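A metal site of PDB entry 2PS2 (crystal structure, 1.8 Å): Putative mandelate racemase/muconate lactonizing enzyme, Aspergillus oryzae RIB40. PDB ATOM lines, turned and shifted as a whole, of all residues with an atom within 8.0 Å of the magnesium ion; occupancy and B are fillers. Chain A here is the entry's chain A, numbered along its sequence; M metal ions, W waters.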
ATOM      1  N   TYR A  60     -11.059 -11.802  15.683  1.00  0.00           N
ATOM      2  CA  TYR A  60     -10.709 -12.552  16.892  1.00  0.00           C
ATOM      3  C   TYR A  60     -11.909 -13.384  17.390  1.00  0.00           C
ATOM      4  O   TYR A  60     -11.848 -14.615  17.471  1.00  0.00           O
ATOM      5  CB  TYR A  60     -10.248 -11.575  17.982  1.00  0.00           C
ATOM      6  CG  TYR A  60      -9.876 -12.224  19.288  1.00  0.00           C
ATOM      7  CD1 TYR A  60      -8.915 -13.241  19.331  1.00  0.00           C
ATOM      8  CD2 TYR A  60     -10.497 -11.849  20.473  1.00  0.00           C
ATOM      9  CE1 TYR A  60      -8.575 -13.857  20.541  1.00  0.00           C
ATOM     10  CE2 TYR A  60     -10.167 -12.457  21.688  1.00  0.00           C
ATOM     11  CZ  TYR A  60      -9.215 -13.468  21.705  1.00  0.00           C
ATOM     12  OH  TYR A  60      -8.900 -14.079  22.894  1.00  0.00           O
ATOM     13  N   SER A 166       3.499 -15.645  26.392  1.00  0.00           N
ATOM     14  CA  SER A 166       2.485 -16.198  25.501  1.00  0.00           C
ATOM     15  C   SER A 166       3.086 -16.317  24.103  1.00  0.00           C
ATOM     16  O   SER A 166       3.340 -15.309  23.436  1.00  0.00           O
ATOM     17  CB  SER A 166       1.252 -15.300  25.472  1.00  0.00           C
ATOM     18  OG  SER A 166       0.245 -15.856  24.638  1.00  0.00           O
ATOM     19  N   LYS A 168       2.723 -17.269  20.308  1.00  0.00           N
ATOM     20  CA  LYS A 168       1.736 -17.459  19.263  1.00  0.00           C
ATOM     21  C   LYS A 168       2.261 -18.376  18.165  1.00  0.00           C
ATOM     22  O   LYS A 168       3.462 -18.418  17.896  1.00  0.00           O
ATOM     23  CB  LYS A 168       1.345 -16.117  18.639  1.00  0.00           C
ATOM     24  CG  LYS A 168       0.950 -15.040  19.643  1.00  0.00           C
ATOM     25  CD  LYS A 168      -0.206 -15.481  20.518  1.00  0.00           C
ATOM     26  CE  LYS A 168      -0.656 -14.366  21.449  1.00  0.00           C
ATOM     27  NZ  LYS A 168       0.421 -13.910  22.367  1.00  0.00           N
ATOM     28  N   ILE A 194       2.690 -20.192  27.796  1.00  0.00           N
ATOM     29  CA  ILE A 194       1.442 -20.492  27.104  1.00  0.00           C
ATOM     30  C   ILE A 194       1.715 -20.501  25.611  1.00  0.00           C
ATOM     31  O   ILE A 194       2.460 -19.649  25.104  1.00  0.00           O
ATOM     32  CB  ILE A 194       0.367 -19.410  27.364  1.00  0.00           C
ATOM     33  CG1 ILE A 194      -0.205 -19.553  28.774  1.00  0.00           C
ATOM     34  CG2 ILE A 194      -0.745 -19.517  26.309  1.00  0.00           C
ATOM     35  CD1 ILE A 194      -1.116 -18.415  29.158  1.00  0.00           C
ATOM     36  N   VAL A 195       1.176 -21.487  24.903  1.00  0.00           N
ATOM     37  CA  VAL A 195       1.303 -21.534  23.451  1.00  0.00           C
ATOM     38  C   VAL A 195      -0.139 -21.253  23.037  1.00  0.00           C
ATOM     39  O   VAL A 195      -1.052 -22.010  23.385  1.00  0.00           O
ATOM     40  CB  VAL A 195       1.749 -22.903  22.933  1.00  0.00           C
ATOM     41  CG1 VAL A 195       1.516 -22.978  21.429  1.00  0.00           C
ATOM     42  CG2 VAL A 195       3.231 -23.107  23.228  1.00  0.00           C
ATOM     43  N   ASP A 196      -0.333 -20.141  22.337  1.00  0.00           N
ATOM     44  CA  ASP A 196      -1.670 -19.713  21.934  1.00  0.00           C
ATOM     45  C   ASP A 196      -1.899 -19.916  20.448  1.00  0.00           C
ATOM     46  O   ASP A 196      -1.268 -19.270  19.617  1.00  0.00           O
ATOM     47  CB  ASP A 196      -1.842 -18.236  22.268  1.00  0.00           C
ATOM     48  CG  ASP A 196      -3.279 -17.808  22.324  1.00  0.00           C
ATOM     49  OD1 ASP A 196      -4.123 -18.396  21.596  1.00  0.00           O
ATOM     50  OD2 ASP A 196      -3.569 -16.888  23.092  1.00  0.00           O
ATOM     51  N   ALA A 197      -2.821 -20.815  20.115  1.00  0.00           N
ATOM     52  CA  ALA A 197      -3.131 -21.116  18.720  1.00  0.00           C
ATOM     53  C   ALA A 197      -4.244 -20.224  18.162  1.00  0.00           C
ATOM     54  O   ALA A 197      -4.495 -20.231  16.960  1.00  0.00           O
ATOM     55  CB  ALA A 197      -3.524 -22.577  18.571  1.00  0.00           C
ATOM     56  N   ASN A 198      -4.884 -19.458  19.039  1.00  0.00           N
ATOM     57  CA  ASN A 198      -5.970 -18.579  18.636  1.00  0.00           C
ATOM     58  C   ASN A 198      -7.006 -19.279  17.760  1.00  0.00           C
ATOM     59  O   ASN A 198      -7.478 -18.713  16.774  1.00  0.00           O
ATOM     60  CB  ASN A 198      -5.410 -17.341  17.922  1.00  0.00           C
ATOM     61  CG  ASN A 198      -4.687 -16.409  18.869  1.00  0.00           C
ATOM     62  OD1 ASN A 198      -3.476 -16.210  18.761  1.00  0.00           O
ATOM     63  ND2 ASN A 198      -5.426 -15.842  19.806  1.00  0.00           N
ATOM     64  N   GLY A 199      -7.324 -20.518  18.127  1.00  0.00           N
ATOM     65  CA  GLY A 199      -8.308 -21.302  17.390  1.00  0.00           C
ATOM     66  C   GLY A 199      -7.948 -21.678  15.959  1.00  0.00           C
ATOM     67  O   GLY A 199      -8.820 -22.095  15.193  1.00  0.00           O
ATOM     68  N   GLU A 222      -3.362 -22.928  24.710  1.00  0.00           N
ATOM     69  CA  GLU A 222      -4.537 -22.071  24.744  1.00  0.00           C
ATOM     70  C   GLU A 222      -5.272 -21.991  23.404  1.00  0.00           C
ATOM     71  O   GLU A 222      -4.644 -21.872  22.357  1.00  0.00           O
ATOM     72  CB  GLU A 222      -4.136 -20.664  25.205  1.00  0.00           C
ATOM     73  CG  GLU A 222      -5.295 -19.687  25.350  1.00  0.00           C
ATOM     74  CD  GLU A 222      -4.910 -18.428  26.113  1.00  0.00           C
ATOM     75  OE1 GLU A 222      -4.326 -18.544  27.208  1.00  0.00           O
ATOM     76  OE2 GLU A 222      -5.219 -17.330  25.632  1.00  0.00           O
ATOM     77  N   ALA A 223      -6.602 -22.075  23.461  1.00  0.00           N
ATOM     78  CA  ALA A 223      -7.442 -21.995  22.263  1.00  0.00           C
ATOM     79  C   ALA A 223      -6.927 -22.807  21.076  1.00  0.00           C
ATOM     80  O   ALA A 223      -6.687 -22.265  19.998  1.00  0.00           O
ATOM     81  CB  ALA A 223      -7.612 -20.533  21.848  1.00  0.00           C
ATOM     82  N   ILE A 243      -6.277 -24.385  27.868  1.00  0.00           N
ATOM     83  CA  ILE A 243      -6.845 -23.150  28.377  1.00  0.00           C
ATOM     84  C   ILE A 243      -7.809 -22.587  27.343  1.00  0.00           C
ATOM     85  O   ILE A 243      -7.449 -22.445  26.172  1.00  0.00           O
ATOM     86  CB  ILE A 243      -5.759 -22.078  28.644  1.00  0.00           C
ATOM     87  CG1 ILE A 243      -4.712 -22.619  29.632  1.00  0.00           C
ATOM     88  CG2 ILE A 243      -6.387 -20.794  29.207  1.00  0.00           C
ATOM     89  CD1 ILE A 243      -5.276 -22.974  30.988  1.00  0.00           C
ATOM     90  N   TYR A 244      -9.026 -22.272  27.765  1.00  0.00           N
ATOM     91  CA  TYR A 244     -10.017 -21.694  26.850  1.00  0.00           C
ATOM     92  C   TYR A 244      -9.892 -20.173  26.851  1.00  0.00           C
ATOM     93  O   TYR A 244      -9.748 -19.573  27.908  1.00  0.00           O
ATOM     94  CB  TYR A 244     -11.437 -22.081  27.286  1.00  0.00           C
ATOM     95  CG  TYR A 244     -11.958 -23.377  26.698  1.00  0.00           C
ATOM     96  CD1 TYR A 244     -11.126 -24.493  26.566  1.00  0.00           C
ATOM     97  CD2 TYR A 244     -13.284 -23.489  26.285  1.00  0.00           C
ATOM     98  CE1 TYR A 244     -11.612 -25.688  26.025  1.00  0.00           C
ATOM     99  CE2 TYR A 244     -13.770 -24.684  25.744  1.00  0.00           C
ATOM    100  CZ  TYR A 244     -12.930 -25.768  25.616  1.00  0.00           C
ATOM    101  OH  TYR A 244     -13.411 -26.942  25.070  1.00  0.00           O
ATOM    102  N   ASP A 245      -9.934 -19.569  25.675  1.00  0.00           N
ATOM    103  CA  ASP A 245      -9.881 -18.124  25.577  1.00  0.00           C
ATOM    104  C   ASP A 245     -11.082 -17.685  24.734  1.00  0.00           C
ATOM    105  O   ASP A 245     -12.122 -17.335  25.279  1.00  0.00           O
ATOM    106  CB  ASP A 245      -8.591 -17.623  24.935  1.00  0.00           C
ATOM    107  CG  ASP A 245      -8.509 -16.096  24.898  1.00  0.00           C
ATOM    108  OD1 ASP A 245      -9.530 -15.434  25.181  1.00  0.00           O
ATOM    109  OD2 ASP A 245      -7.446 -15.542  24.571  1.00  0.00           O
ATOM    110  N   GLU A 246     -10.948 -17.756  23.412  1.00  0.00           N
ATOM    111  CA  GLU A 246     -12.044 -17.348  22.535  1.00  0.00           C
ATOM    112  C   GLU A 246     -13.384 -18.003  22.881  1.00  0.00           C
ATOM    113  O   GLU A 246     -14.434 -17.363  22.790  1.00  0.00           O
ATOM    114  CB  GLU A 246     -11.712 -17.641  21.070  1.00  0.00           C
ATOM    115  CG  GLU A 246     -10.734 -16.659  20.435  1.00  0.00           C
ATOM    116  CD  GLU A 246      -9.286 -17.085  20.589  1.00  0.00           C
ATOM    117  OE1 GLU A 246      -8.857 -17.345  21.721  1.00  0.00           O
ATOM    118  OE2 GLU A 246      -8.578 -17.141  19.555  1.00  0.00           O
ATOM    119  N   ASP A 267      -8.617 -17.900  29.943  1.00  0.00           N
ATOM    120  CA  ASP A 267      -7.961 -16.610  29.724  1.00  0.00           C
ATOM    121  C   ASP A 267      -9.181 -15.702  29.838  1.00  0.00           C
ATOM    122  O   ASP A 267     -10.003 -15.622  28.907  1.00  0.00           O
ATOM    123  CB  ASP A 267      -7.378 -16.525  28.314  1.00  0.00           C
ATOM    124  CG  ASP A 267      -6.604 -15.240  28.069  1.00  0.00           C
ATOM    125  OD1 ASP A 267      -6.942 -14.202  28.688  1.00  0.00           O
ATOM    126  OD2 ASP A 267      -5.669 -15.257  27.249  1.00  0.00           O
ATOM    127  N   LYS A 269     -10.764 -12.425  29.554  1.00  0.00           N
ATOM    128  CA  LYS A 269     -10.613 -11.091  28.997  1.00  0.00           C
ATOM    129  C   LYS A 269     -11.843 -10.300  29.393  1.00  0.00           C
ATOM    130  O   LYS A 269     -12.974 -10.706  29.119  1.00  0.00           O
ATOM    131  CB  LYS A 269     -10.445 -11.173  27.470  1.00  0.00           C
ATOM    132  CG  LYS A 269      -9.069 -11.721  27.114  1.00  0.00           C
ATOM    133  CD  LYS A 269      -8.855 -11.924  25.638  1.00  0.00           C
ATOM    134  CE  LYS A 269      -7.450 -12.451  25.405  1.00  0.00           C
ATOM    135  NZ  LYS A 269      -7.160 -12.610  23.951  1.00  0.00           N
ATOM    136  N   LYS A 272     -14.576  -9.700  26.887  1.00  0.00           N
ATOM    137  CA  LYS A 272     -15.137 -10.915  26.306  1.00  0.00           C
ATOM    138  C   LYS A 272     -16.063 -11.537  27.363  1.00  0.00           C
ATOM    139  O   LYS A 272     -17.074 -12.164  27.041  1.00  0.00           O
ATOM    140  CB  LYS A 272     -14.029 -11.916  25.922  1.00  0.00           C
ATOM    141  CG  LYS A 272     -14.564 -13.305  25.532  1.00  0.00           C
ATOM    142  CD  LYS A 272     -13.599 -14.071  24.607  1.00  0.00           C
ATOM    143  CE  LYS A 272     -12.190 -14.180  25.167  1.00  0.00           C
ATOM    144  NZ  LYS A 272     -12.104 -14.912  26.461  1.00  0.00           N
ATOM    145  N   GLN A 296      -6.829 -10.774  31.172  1.00  0.00           N
ATOM    146  CA  GLN A 296      -6.320 -10.011  30.049  1.00  0.00           C
ATOM    147  C   GLN A 296      -7.436  -9.197  29.416  1.00  0.00           C
ATOM    148  O   GLN A 296      -8.475  -8.945  30.023  1.00  0.00           O
ATOM    149  CB  GLN A 296      -5.709 -10.953  29.008  1.00  0.00           C
ATOM    150  CG  GLN A 296      -4.589 -11.838  29.565  1.00  0.00           C
ATOM    151  CD  GLN A 296      -3.916 -12.677  28.503  1.00  0.00           C
ATOM    152  OE1 GLN A 296      -3.874 -12.302  27.335  1.00  0.00           O
ATOM    153  NE2 GLN A 296      -3.371 -13.821  28.910  1.00  0.00           N
ATOM    154  N   GLU A 297      -7.221  -8.795  28.164  1.00  0.00           N
ATOM    155  CA  GLU A 297      -8.222  -8.036  27.442  1.00  0.00           C
ATOM    156  C   GLU A 297      -8.004  -8.293  25.962  1.00  0.00           C
ATOM    157  O   GLU A 297      -6.923  -8.705  25.558  1.00  0.00           O
ATOM    158  CB  GLU A 297      -8.060  -6.539  27.768  1.00  0.00           C
ATOM    159  CG  GLU A 297      -9.099  -5.618  27.160  1.00  0.00           C
ATOM    160  CD  GLU A 297     -10.524  -5.978  27.543  1.00  0.00           C
ATOM    161  OE1 GLU A 297     -10.954  -7.094  27.182  1.00  0.00           O
ATOM    162  OE2 GLU A 297     -11.207  -5.167  28.185  1.00  0.00           O
HETATM  163 MG    MG M   1      -5.508 -16.231  23.760  1.00  0.00          MG
HETATM  164  O   HOH W   1      -6.460 -17.470  22.515  1.00  0.00           O
HETATM  165  O   HOH W   2      -4.668 -14.459  24.864  1.00  0.00           O
HETATM  166  O   HOH W   3      -5.778 -15.098  22.102  1.00  0.00           O
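The backbone carbonyl oxygen (O) of Glu 222 sits at hydrogen-bond distance from the backbone NH (N) of Ala 197, 3.1 Å away. O of Asp 267 is in hydrogen-bond range of NZ of Lys 272 (3.3 Å). The backbone carbonyl oxygen (O) of Ala 223 lies within hydrogen-bond range of the backbone NH (N) of Asn 198. The side-chain carboxylate (OE2) of Glu 222 sits close to the side-chain carboxylate (OD2) of Asp 267, at 2.7 Å. The side-chain carboxylate (OD1) of Asp 245 is in salt-bridge range of the side-chain amino group (NZ) of Lys 269 (3.9 Å). The side-chain carboxylate (OE2) of Glu 246 sits close to the side-chain amide nitrogen (ND2) of Asn 198, at 3.4 Å. The backbone NH of Asp 267 sits at hydrogen-bond distance from the backbone carbonyl oxygen of Tyr 244. The side-chain carboxylate (OD1) of Asp 196 is in hydrogen-bond range of the backbone NH (N) of Asn 198 (2.9 Å).
Residues that only touch the magnesium ion: Asn 198, Asp 267 and Lys 269. Six residues have an atom within 4 Å of the magnesium ion: Asp 196, Asn 198, Glu 222, Asp 245, Asp 267 and Lys 269.
The magnesium ion is bound by water W1 (2.0 Å), water W3 (2.0 Å), the side-chain carboxylate of Asp 196 (2.2 Å), the side-chain carboxylate of Glu 222 (2.2 Å), the side-chain carboxylate of Asp 245 (2.2 Å) and water W2 (2.3 Å). The magnesium ion has six donor atoms within binding distance.
Water W1 lies within hydrogen-bond range of OE1 of Glu 246 (2.5 Å), OD1 of Asp 196 (2.7 Å) and ND2 of Asn 198 (3.3 Å). Water W3 lies within hydrogen-bond range of ND2 of Asn 198 (2.4 Å), OH of Tyr 60 (3.4 Å) and NZ of Lys 269 (3.4 Å). Water W2 lies within hydrogen-bond range of the side-chain carboxylate (OD2) of Asp 267 (2.7 Å), the side-chain amino group (NZ) of Lys 269 (3.2 Å) and the side-chain amide oxygen (OE1) of Gln 296 (3.4 Å).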
